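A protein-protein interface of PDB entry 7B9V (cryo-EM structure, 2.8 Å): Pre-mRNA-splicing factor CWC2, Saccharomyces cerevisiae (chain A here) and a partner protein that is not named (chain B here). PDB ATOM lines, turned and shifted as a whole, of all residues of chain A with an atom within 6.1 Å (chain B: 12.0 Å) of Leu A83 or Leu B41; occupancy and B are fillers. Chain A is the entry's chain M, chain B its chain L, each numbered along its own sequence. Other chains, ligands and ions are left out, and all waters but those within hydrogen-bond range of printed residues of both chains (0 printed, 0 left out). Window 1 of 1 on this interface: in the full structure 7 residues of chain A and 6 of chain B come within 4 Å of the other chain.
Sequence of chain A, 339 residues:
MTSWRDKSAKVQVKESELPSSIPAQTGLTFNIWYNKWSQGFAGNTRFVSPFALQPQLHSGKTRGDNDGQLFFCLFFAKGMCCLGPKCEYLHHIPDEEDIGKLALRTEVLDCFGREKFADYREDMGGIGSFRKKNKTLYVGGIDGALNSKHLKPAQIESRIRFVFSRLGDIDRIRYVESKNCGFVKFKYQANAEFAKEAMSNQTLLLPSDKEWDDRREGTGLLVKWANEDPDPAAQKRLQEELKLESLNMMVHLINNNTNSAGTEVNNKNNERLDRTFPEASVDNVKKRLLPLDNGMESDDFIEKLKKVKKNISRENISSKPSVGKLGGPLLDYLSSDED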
ATOM      1  N   LYS A  10      19.544  15.136  29.373  1.00  0.00           N
ATOM      2  CA  LYS A  10      18.588  16.034  29.999  1.00  0.00           C
ATOM      3  C   LYS A  10      17.811  16.819  28.951  1.00  0.00           C
ATOM      4  O   LYS A  10      18.348  17.189  27.904  1.00  0.00           O
ATOM      5  CB  LYS A  10      19.318  16.990  30.943  1.00  0.00           C
ATOM      6  CG  LYS A  10      18.449  17.581  32.034  1.00  0.00           C
ATOM      7  CD  LYS A  10      18.273  16.598  33.181  1.00  0.00           C
ATOM      8  CE  LYS A  10      17.435  17.198  34.296  1.00  0.00           C
ATOM      9  NZ  LYS A  10      17.321  16.280  35.461  1.00  0.00           N
ATOM     10  N   VAL A  11      16.535  17.067  29.237  1.00  0.00           N
ATOM     11  CA  VAL A  11      15.760  17.995  28.428  1.00  0.00           C
ATOM     12  C   VAL A  11      16.230  19.404  28.759  1.00  0.00           C
ATOM     13  O   VAL A  11      16.125  19.853  29.906  1.00  0.00           O
ATOM     14  CB  VAL A  11      14.257  17.828  28.672  1.00  0.00           C
ATOM     15  CG1 VAL A  11      13.486  18.940  27.985  1.00  0.00           C
ATOM     16  CG2 VAL A  11      13.798  16.473  28.176  1.00  0.00           C
ATOM     17  N   VAL A  13      15.224  22.474  27.249  1.00  0.00           N
ATOM     18  CA  VAL A  13      14.130  23.447  27.243  1.00  0.00           C
ATOM     19  C   VAL A  13      12.832  22.698  26.965  1.00  0.00           C
ATOM     20  O   VAL A  13      12.787  21.834  26.083  1.00  0.00           O
ATOM     21  CB  VAL A  13      14.362  24.553  26.172  1.00  0.00           C
ATOM     22  CG1 VAL A  13      13.251  25.561  26.133  1.00  0.00           C
ATOM     23  CG2 VAL A  13      15.596  25.346  26.455  1.00  0.00           C
ATOM     24  N   GLU A  15       8.953  22.229  25.590  1.00  0.00           N
ATOM     25  CA  GLU A  15       8.258  22.647  24.368  1.00  0.00           C
ATOM     26  C   GLU A  15       7.500  23.960  24.566  1.00  0.00           C
ATOM     27  O   GLU A  15       7.478  24.818  23.673  1.00  0.00           O
ATOM     28  CB  GLU A  15       7.305  21.532  23.919  1.00  0.00           C
ATOM     29  CG  GLU A  15       6.227  21.881  22.865  1.00  0.00           C
ATOM     30  CD  GLU A  15       6.775  22.329  21.498  1.00  0.00           C
ATOM     31  OE1 GLU A  15       7.955  22.067  21.170  1.00  0.00           O
ATOM     32  OE2 GLU A  15       6.009  22.954  20.736  1.00  0.00           O
ATOM     33  N   LEU A  18       9.952  27.054  24.586  1.00  0.00           N
ATOM     34  CA  LEU A  18      10.664  27.438  23.374  1.00  0.00           C
ATOM     35  C   LEU A  18      10.264  28.836  22.885  1.00  0.00           C
ATOM     36  O   LEU A  18       9.109  29.250  23.045  1.00  0.00           O
ATOM     37  CB  LEU A  18      10.430  26.402  22.272  1.00  0.00           C
ATOM     38  CG  LEU A  18      11.075  25.030  22.436  1.00  0.00           C
ATOM     39  CD1 LEU A  18      10.660  24.178  21.273  1.00  0.00           C
ATOM     40  CD2 LEU A  18      12.588  25.151  22.465  1.00  0.00           C
ATOM     41  N   CYS A  81      17.612  22.202  22.952  1.00  0.00           N
ATOM     42  CA  CYS A  81      16.925  21.005  22.469  1.00  0.00           C
ATOM     43  C   CYS A  81      15.709  20.634  23.307  1.00  0.00           C
ATOM     44  O   CYS A  81      15.799  20.454  24.524  1.00  0.00           O
ATOM     45  CB  CYS A  81      17.863  19.812  22.406  1.00  0.00           C
ATOM     46  SG  CYS A  81      17.020  18.474  21.505  1.00  0.00           S
ATOM     47  N   CYS A  82      14.575  20.501  22.623  1.00  0.00           N
ATOM     48  CA  CYS A  82      13.287  20.160  23.214  1.00  0.00           C
ATOM     49  C   CYS A  82      13.110  18.660  23.496  1.00  0.00           C
ATOM     50  O   CYS A  82      12.419  18.293  24.454  1.00  0.00           O
ATOM     51  CB  CYS A  82      12.207  20.693  22.274  1.00  0.00           C
ATOM     52  SG  CYS A  82      10.528  20.263  22.661  1.00  0.00           S
ATOM     53  N   LEU A  83      13.718  17.794  22.685  1.00  0.00           N
ATOM     54  CA  LEU A  83      13.459  16.350  22.701  1.00  0.00           C
ATOM     55  C   LEU A  83      14.252  15.564  23.740  1.00  0.00           C
ATOM     56  O   LEU A  83      13.757  14.511  24.167  1.00  0.00           O
ATOM     57  CB  LEU A  83      13.689  15.744  21.313  1.00  0.00           C
ATOM     58  CG  LEU A  83      12.877  16.364  20.172  1.00  0.00           C
ATOM     59  CD1 LEU A  83      13.058  15.549  18.907  1.00  0.00           C
ATOM     60  CD2 LEU A  83      11.400  16.431  20.545  1.00  0.00           C
ATOM     61  N   GLY A  84      15.370  16.111  24.238  1.00  0.00           N
ATOM     62  CA  GLY A  84      16.185  15.496  25.272  1.00  0.00           C
ATOM     63  C   GLY A  84      16.624  14.089  24.914  1.00  0.00           C
ATOM     64  O   GLY A  84      17.393  13.900  23.970  1.00  0.00           O
ATOM     65  N   PRO A  85      16.176  13.071  25.653  1.00  0.00           N
ATOM     66  CA  PRO A  85      16.634  11.715  25.345  1.00  0.00           C
ATOM     67  C   PRO A  85      15.932  11.095  24.150  1.00  0.00           C
ATOM     68  O   PRO A  85      16.470  10.141  23.576  1.00  0.00           O
ATOM     69  CB  PRO A  85      16.323  10.947  26.632  1.00  0.00           C
ATOM     70  CG  PRO A  85      15.105  11.616  27.148  1.00  0.00           C
ATOM     71  CD  PRO A  85      15.295  13.087  26.834  1.00  0.00           C
ATOM     72  N   LYS A  86      14.755  11.594  23.756  1.00  0.00           N
ATOM     73  CA  LYS A  86      14.066  11.114  22.562  1.00  0.00           C
ATOM     74  C   LYS A  86      14.647  11.674  21.260  1.00  0.00           C
ATOM     75  O   LYS A  86      14.075  11.432  20.192  1.00  0.00           O
ATOM     76  CB  LYS A  86      12.577  11.466  22.641  1.00  0.00           C
ATOM     77  CG  LYS A  86      11.866  11.037  23.922  1.00  0.00           C
ATOM     78  CD  LYS A  86      11.888   9.525  24.111  1.00  0.00           C
ATOM     79  CE  LYS A  86      11.003   9.106  25.280  1.00  0.00           C
ATOM     80  NZ  LYS A  86      11.271   7.715  25.741  1.00  0.00           N
ATOM     81  N   CYS A  87      15.723  12.454  21.334  1.00  0.00           N
ATOM     82  CA  CYS A  87      16.317  13.088  20.163  1.00  0.00           C
ATOM     83  C   CYS A  87      16.995  12.073  19.250  1.00  0.00           C
ATOM     84  O   CYS A  87      17.705  11.180  19.717  1.00  0.00           O
ATOM     85  CB  CYS A  87      17.327  14.141  20.596  1.00  0.00           C
ATOM     86  SG  CYS A  87      17.614  15.365  19.309  1.00  0.00           S
ATOM     87  N   GLU A  88      16.780  12.217  17.936  1.00  0.00           N
ATOM     88  CA  GLU A  88      17.476  11.376  16.963  1.00  0.00           C
ATOM     89  C   GLU A  88      18.969  11.680  16.840  1.00  0.00           C
ATOM     90  O   GLU A  88      19.685  10.913  16.197  1.00  0.00           O
ATOM     91  CB  GLU A  88      16.844  11.534  15.581  1.00  0.00           C
ATOM     92  CG  GLU A  88      15.337  11.372  15.539  1.00  0.00           C
ATOM     93  CD  GLU A  88      14.594  12.699  15.606  1.00  0.00           C
ATOM     94  OE1 GLU A  88      14.884  13.505  16.518  1.00  0.00           O
ATOM     95  OE2 GLU A  88      13.710  12.929  14.756  1.00  0.00           O
ATOM     96  N   HIS A  91      23.612  13.973  21.675  1.00  0.00           N
ATOM     97  CA  HIS A  91      23.728  14.994  22.726  1.00  0.00           C
ATOM     98  C   HIS A  91      25.006  14.821  23.546  1.00  0.00           C
ATOM     99  O   HIS A  91      24.938  14.518  24.737  1.00  0.00           O
ATOM    100  CB  HIS A  91      22.526  14.953  23.653  1.00  0.00           C
ATOM    101  CG  HIS A  91      21.308  15.593  23.090  1.00  0.00           C
ATOM    102  ND1 HIS A  91      20.364  16.208  23.881  1.00  0.00           N
ATOM    103  CD2 HIS A  91      20.863  15.694  21.818  1.00  0.00           C
ATOM    104  CE1 HIS A  91      19.397  16.679  23.117  1.00  0.00           C
ATOM    105  NE2 HIS A  91      19.673  16.375  21.862  1.00  0.00           N
ATOM    106  N   LYS B  35      -7.577  20.163  18.010  1.00  0.00           N
ATOM    107  CA  LYS B  35      -7.346  21.595  18.059  1.00  0.00           C
ATOM    108  C   LYS B  35      -5.930  21.964  17.624  1.00  0.00           C
ATOM    109  O   LYS B  35      -5.005  21.149  17.642  1.00  0.00           O
ATOM    110  CB  LYS B  35      -7.645  22.137  19.452  1.00  0.00           C
ATOM    111  CG  LYS B  35      -9.109  22.020  19.802  1.00  0.00           C
ATOM    112  CD  LYS B  35      -9.413  22.614  21.152  1.00  0.00           C
ATOM    113  CE  LYS B  35     -10.907  22.602  21.407  1.00  0.00           C
ATOM    114  NZ  LYS B  35     -11.247  23.208  22.719  1.00  0.00           N
ATOM    115  N   ASP B  36      -5.775  23.232  17.255  1.00  0.00           N
ATOM    116  CA  ASP B  36      -4.490  23.823  16.884  1.00  0.00           C
ATOM    117  C   ASP B  36      -3.694  24.064  18.167  1.00  0.00           C
ATOM    118  O   ASP B  36      -3.777  25.128  18.782  1.00  0.00           O
ATOM    119  CB  ASP B  36      -4.701  25.110  16.087  1.00  0.00           C
ATOM    120  CG  ASP B  36      -3.396  25.736  15.569  1.00  0.00           C
ATOM    121  OD1 ASP B  36      -2.294  25.149  15.683  1.00  0.00           O
ATOM    122  OD2 ASP B  36      -3.485  26.863  15.041  1.00  0.00           O
ATOM    123  N   LYS B  37      -2.900  23.076  18.575  1.00  0.00           N
ATOM    124  CA  LYS B  37      -1.999  23.277  19.705  1.00  0.00           C
ATOM    125  C   LYS B  37      -0.745  24.071  19.348  1.00  0.00           C
ATOM    126  O   LYS B  37       0.028  24.396  20.258  1.00  0.00           O
ATOM    127  CB  LYS B  37      -1.586  21.936  20.314  1.00  0.00           C
ATOM    128  CG  LYS B  37      -2.739  21.071  20.776  1.00  0.00           C
ATOM    129  CD  LYS B  37      -3.442  21.685  21.980  1.00  0.00           C
ATOM    130  CE  LYS B  37      -4.461  20.716  22.566  1.00  0.00           C
ATOM    131  NZ  LYS B  37      -5.209  21.272  23.729  1.00  0.00           N
ATOM    132  N   SER B  38      -0.523  24.331  18.054  1.00  0.00           N
ATOM    133  CA  SER B  38       0.536  25.199  17.511  1.00  0.00           C
ATOM    134  C   SER B  38       1.931  24.673  17.848  1.00  0.00           C
ATOM    135  O   SER B  38       2.764  25.383  18.423  1.00  0.00           O
ATOM    136  CB  SER B  38       0.376  26.661  17.957  1.00  0.00           C
ATOM    137  OG  SER B  38      -0.913  27.161  17.657  1.00  0.00           O
ATOM    138  N   SER B  39       2.135  23.380  17.583  1.00  0.00           N
ATOM    139  CA  SER B  39       3.450  22.777  17.742  1.00  0.00           C
ATOM    140  C   SER B  39       4.452  23.432  16.801  1.00  0.00           C
ATOM    141  O   SER B  39       4.146  23.734  15.645  1.00  0.00           O
ATOM    142  CB  SER B  39       3.371  21.270  17.478  1.00  0.00           C
ATOM    143  OG  SER B  39       4.654  20.699  17.271  1.00  0.00           O
ATOM    144  N   LYS B  40       5.662  23.655  17.309  1.00  0.00           N
ATOM    145  CA  LYS B  40       6.734  24.297  16.557  1.00  0.00           C
ATOM    146  C   LYS B  40       7.525  23.317  15.693  1.00  0.00           C
ATOM    147  O   LYS B  40       7.898  23.630  14.555  1.00  0.00           O
ATOM    148  CB  LYS B  40       7.654  25.048  17.520  1.00  0.00           C
ATOM    149  CG  LYS B  40       8.691  25.901  16.825  1.00  0.00           C
ATOM    150  CD  LYS B  40       9.528  26.716  17.796  1.00  0.00           C
ATOM    151  CE  LYS B  40      10.474  27.611  17.016  1.00  0.00           C
ATOM    152  NZ  LYS B  40      11.408  28.394  17.867  1.00  0.00           N
ATOM    153  N   LEU B  41       7.761  22.132  16.238  1.00  0.00           N
ATOM    154  CA  LEU B  41       8.547  21.057  15.645  1.00  0.00           C
ATOM    155  C   LEU B  41       7.715  20.204  14.690  1.00  0.00           C
ATOM    156  O   LEU B  41       6.516  20.004  14.885  1.00  0.00           O
ATOM    157  CB  LEU B  41       9.174  20.209  16.762  1.00  0.00           C
ATOM    158  CG  LEU B  41      10.442  20.672  17.521  1.00  0.00           C
ATOM    159  CD1 LEU B  41      10.342  21.950  18.328  1.00  0.00           C
ATOM    160  CD2 LEU B  41      10.867  19.555  18.452  1.00  0.00           C
ATOM    161  N   ALA B  42       8.380  19.681  13.652  1.00  0.00           N
ATOM    162  CA  ALA B  42       7.751  18.700  12.766  1.00  0.00           C
ATOM    163  C   ALA B  42       7.461  17.377  13.466  1.00  0.00           C
ATOM    164  O   ALA B  42       6.401  16.778  13.234  1.00  0.00           O
ATOM    165  CB  ALA B  42       8.637  18.472  11.538  1.00  0.00           C
ATOM    166  N   ALA B  43       8.425  16.870  14.246  1.00  0.00           N
ATOM    167  CA  ALA B  43       8.276  15.611  14.994  1.00  0.00           C
ATOM    168  C   ALA B  43       7.052  15.598  15.918  1.00  0.00           C
ATOM    169  O   ALA B  43       6.214  14.680  15.863  1.00  0.00           O
ATOM    170  CB  ALA B  43       9.551  15.330  15.790  1.00  0.00           C
ATOM    171  N   LYS B  44       6.922  16.620  16.763  1.00  0.00           N
ATOM    172  CA  LYS B  44       5.796  16.704  17.690  1.00  0.00           C
ATOM    173  C   LYS B  44       4.477  17.022  16.990  1.00  0.00           C
ATOM    174  O   LYS B  44       3.416  16.514  17.419  1.00  0.00           O
ATOM    175  CB  LYS B  44       6.113  17.753  18.756  1.00  0.00           C
ATOM    176  CG  LYS B  44       7.110  17.272  19.803  1.00  0.00           C
ATOM    177  CD  LYS B  44       7.248  18.261  20.935  1.00  0.00           C
ATOM    178  CE  LYS B  44       8.102  17.685  22.043  1.00  0.00           C
ATOM    179  NZ  LYS B  44       7.466  16.545  22.749  1.00  0.00           N
ATOM    180  N   SER B  45       4.553  17.641  15.802  1.00  0.00           N
ATOM    181  CA  SER B  45       3.356  17.815  14.987  1.00  0.00           C
ATOM    182  C   SER B  45       2.896  16.482  14.419  1.00  0.00           C
ATOM    183  O   SER B  45       1.688  16.265  14.270  1.00  0.00           O
ATOM    184  CB  SER B  45       3.632  18.803  13.850  1.00  0.00           C
ATOM    185  OG  SER B  45       3.945  20.094  14.341  1.00  0.00           O
ATOM    186  N   ASN B  46       3.836  15.597  14.058  1.00  0.00           N
ATOM    187  CA  ASN B  46       3.437  14.264  13.604  1.00  0.00           C
ATOM    188  C   ASN B  46       2.806  13.468  14.741  1.00  0.00           C
ATOM    189  O   ASN B  46       1.848  12.709  14.511  1.00  0.00           O
ATOM    190  CB  ASN B  46       4.630  13.512  13.023  1.00  0.00           C
ATOM    191  CG  ASN B  46       5.060  14.056  11.683  1.00  0.00           C
ATOM    192  OD1 ASN B  46       4.273  14.679  10.975  1.00  0.00           O
ATOM    193  ND2 ASN B  46       6.317  13.826  11.329  1.00  0.00           N
ATOM    194  N   GLU B  47       3.362  13.605  15.964  1.00  0.00           N
ATOM    195  CA  GLU B  47       2.855  12.882  17.142  1.00  0.00           C
ATOM    196  C   GLU B  47       1.386  13.204  17.419  1.00  0.00           C
ATOM    197  O   GLU B  47       0.614  12.331  17.858  1.00  0.00           O
ATOM    198  CB  GLU B  47       3.706  13.200  18.369  1.00  0.00           C
ATOM    199  CG  GLU B  47       5.105  12.616  18.319  1.00  0.00           C
ATOM    200  CD  GLU B  47       5.929  12.986  19.530  1.00  0.00           C
ATOM    201  OE1 GLU B  47       5.376  13.614  20.455  1.00  0.00           O
ATOM    202  OE2 GLU B  47       7.132  12.652  19.551  1.00  0.00           O
ATOM    203  N   GLN B  48       0.977  14.444  17.118  1.00  0.00           N
ATOM    204  CA  GLN B  48      -0.401  14.837  17.404  1.00  0.00           C
ATOM    205  C   GLN B  48      -1.398  14.197  16.428  1.00  0.00           C
ATOM    206  O   GLN B  48      -2.540  13.928  16.813  1.00  0.00           O
ATOM    207  CB  GLN B  48      -0.535  16.351  17.398  1.00  0.00           C
ATOM    208  CG  GLN B  48       0.239  16.996  18.520  1.00  0.00           C
ATOM    209  CD  GLN B  48       0.100  18.493  18.537  1.00  0.00           C
ATOM    210  OE1 GLN B  48      -0.800  19.054  17.916  1.00  0.00           O
ATOM    211  NE2 GLN B  48       0.994  19.156  19.254  1.00  0.00           N
ATOM    212  N   LEU B  49      -0.986  13.929  15.179  1.00  0.00           N
ATOM    213  CA  LEU B  49      -1.815  13.152  14.248  1.00  0.00           C
ATOM    214  C   LEU B  49      -1.830  11.673  14.614  1.00  0.00           C
ATOM    215  O   LEU B  49      -2.839  10.977  14.371  1.00  0.00           O
ATOM    216  CB  LEU B  49      -1.302  13.334  12.821  1.00  0.00           C
ATOM    217  CG  LEU B  49      -1.381  14.740  12.235  1.00  0.00           C
ATOM    218  CD1 LEU B  49      -0.486  14.873  11.033  1.00  0.00           C
ATOM    219  CD2 LEU B  49      -2.807  14.982  11.810  1.00  0.00           C
ATOM    220  N   TRP B  50      -0.696  11.170  15.129  1.00  0.00           N
ATOM    221  CA  TRP B  50      -0.630   9.795  15.630  1.00  0.00           C
ATOM    222  C   TRP B  50      -1.642   9.560  16.745  1.00  0.00           C
ATOM    223  O   TRP B  50      -2.188   8.452  16.874  1.00  0.00           O
ATOM    224  CB  TRP B  50       0.780   9.465  16.125  1.00  0.00           C
ATOM    225  CG  TRP B  50       1.896   9.557  15.124  1.00  0.00           C
ATOM    226  CD1 TRP B  50       1.787   9.739  13.779  1.00  0.00           C
ATOM    227  CD2 TRP B  50       3.301   9.489  15.406  1.00  0.00           C
ATOM    228  NE1 TRP B  50       3.028   9.757  13.201  1.00  0.00           N
ATOM    229  CE2 TRP B  50       3.975   9.595  14.176  1.00  0.00           C
ATOM    230  CE3 TRP B  50       4.049   9.289  16.572  1.00  0.00           C
ATOM    231  CZ2 TRP B  50       5.363   9.549  14.080  1.00  0.00           C
ATOM    232  CZ3 TRP B  50       5.426   9.242  16.475  1.00  0.00           C
ATOM    233  CH2 TRP B  50       6.069   9.373  15.238  1.00  0.00           C
ATOM    234  N   HIS B 143      11.423   2.660  15.984  1.00  0.00           N
ATOM    235  CA  HIS B 143      10.619   2.974  17.163  1.00  0.00           C
ATOM    236  C   HIS B 143       9.138   3.145  16.829  1.00  0.00           C
ATOM    237  O   HIS B 143       8.295   2.405  17.344  1.00  0.00           O
ATOM    238  CB  HIS B 143      11.178   4.227  17.840  1.00  0.00           C
ATOM    239  CG  HIS B 143      12.654   4.162  18.080  1.00  0.00           C
ATOM    240  ND1 HIS B 143      13.212   3.450  19.119  1.00  0.00           N
ATOM    241  CD2 HIS B 143      13.686   4.718  17.405  1.00  0.00           C
ATOM    242  CE1 HIS B 143      14.527   3.570  19.072  1.00  0.00           C
ATOM    243  NE2 HIS B 143      14.840   4.335  18.043  1.00  0.00           N
ATOM    244  N   GLN B 144       8.809   4.101  15.955  1.00  0.00           N
ATOM    245  CA  GLN B 144       7.430   4.428  15.608  1.00  0.00           C
ATOM    246  C   GLN B 144       7.346   4.755  14.130  1.00  0.00           C
ATOM    247  O   GLN B 144       8.194   5.476  13.596  1.00  0.00           O
ATOM    248  CB  GLN B 144       6.910   5.630  16.402  1.00  0.00           C
ATOM    249  CG  GLN B 144       6.465   5.288  17.790  1.00  0.00           C
ATOM    250  CD  GLN B 144       6.034   6.470  18.623  1.00  0.00           C
ATOM    251  OE1 GLN B 144       6.847   7.301  19.019  1.00  0.00           O
ATOM    252  NE2 GLN B 144       4.738   6.545  18.902  1.00  0.00           N
ATOM    253  N   ARG B 151       3.869   1.077  16.992  1.00  0.00           N
ATOM    254  CA  ARG B 151       5.158   0.522  17.375  1.00  0.00           C
ATOM    255  C   ARG B 151       5.276  -0.951  17.043  1.00  0.00           C
ATOM    256  O   ARG B 151       6.267  -1.583  17.417  1.00  0.00           O
ATOM    257  CB  ARG B 151       5.376   0.726  18.872  1.00  0.00           C
ATOM    258  CG  ARG B 151       5.468   2.167  19.279  1.00  0.00           C
ATOM    259  CD  ARG B 151       5.628   2.303  20.757  1.00  0.00           C
ATOM    260  NE  ARG B 151       5.784   3.657  21.276  1.00  0.00           N
ATOM    261  CZ  ARG B 151       6.955   4.234  21.511  1.00  0.00           C
ATOM    262  NH1 ARG B 151       8.093   3.609  21.266  1.00  0.00           N
ATOM    263  NH2 ARG B 151       6.982   5.456  22.033  1.00  0.00           N
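Of the 19 printed residues of chain B, 4 touch a printed residue of chain A. Hydrophobic or aromatic side chains of chain B that line the printed part of chain A: Leu B41. Along chain B the printed residues that touch a printed residue of chain A span positions 39 to 44. Of the 14 printed residues of chain A, 4 touch a printed residue of chain B. Hydrophobic or aromatic side chains of chain A that line the printed part of chain B: Leu A18 and Leu A83. Among the printed residues, 8 pairs touch across the chains. Among the printed residues, no Asp or Glu carboxylate lies within 4 Å of a Lys or Arg side-chain nitrogen of the other chain.
SG of Cys A81 lies close to N of Leu A83 (3.6 Å). The side-chain hydroxyl (OG) of Ser B39 sits at hydrogen-bond distance from the backbone carbonyl oxygen (O) of Leu B41. The side-chain hydroxyl of Ser B39 sits at hydrogen-bond distance from the side-chain hydroxyl of Ser B45 (3.1 Å). The backbone carbonyl oxygen (O) of Leu B41 sits at hydrogen-bond distance from the side-chain hydroxyl (OG) of Ser B45, at 2.6 Å. The side-chain carboxylate (OE1) of Glu A15 sits at hydrogen-bond distance from the side-chain sulfur (SG) of Cys A82, 3.5 Å away.
No residue of chain B comes within 4 Å of Val A11. Val A13 touches none of the printed residues of chain B. Of chain B, only Ser B39 (3.9 Å), Lys B40 (3.5 Å), Leu B41 (3.7 Å) and Lys B44 (3.9 Å) come within 4 Å of Glu A15. No residue of chain B comes within 4 Å of Cys A81. Of chain B, only Leu B41 (3.8 Å) and Lys B44 (3.8 Å) come within 4 Å of Leu A83. No residue of chain B comes within 4 Å of Gly A84. No residue of chain B comes within 4 Å of Lys A86. No residue of chain B comes within 4 Å of Cys A87. Of the printed residues of chain A, Ser B39 touches Glu A15. Leu B41 touches just these residues of chain A: Glu A15 (3.7 Å), Leu A18 (3.7 Å) and Leu A83 (3.8 Å). Of the printed residues of chain A, Lys B44 touches Glu A15 (3.9 Å), Cys A82 (3.6 Å) and Leu A83 (3.8 Å). Glu B47 touches none of the printed residues of chain A. The nearest residue of chain B that does not touch Leu A83 is Ala B43 (4.7 Å). The nearest residue of chain A that does not touch Leu B41 is Cys A82 (4.2 Å). The nearest printed residue of chain A that does not touch Ser B39 is Leu A18 (7.7 Å).
Among the printed residues, merely in contact across the chains: Glu A15 with Lys B40, Cys A82 with Lys B44, Leu A18 with Leu B41, Glu A15 with Leu B41, Leu A83 with Leu B41, Leu A83 with Lys B44, Glu A15 with Lys B44 and Glu A15 with Ser B39.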
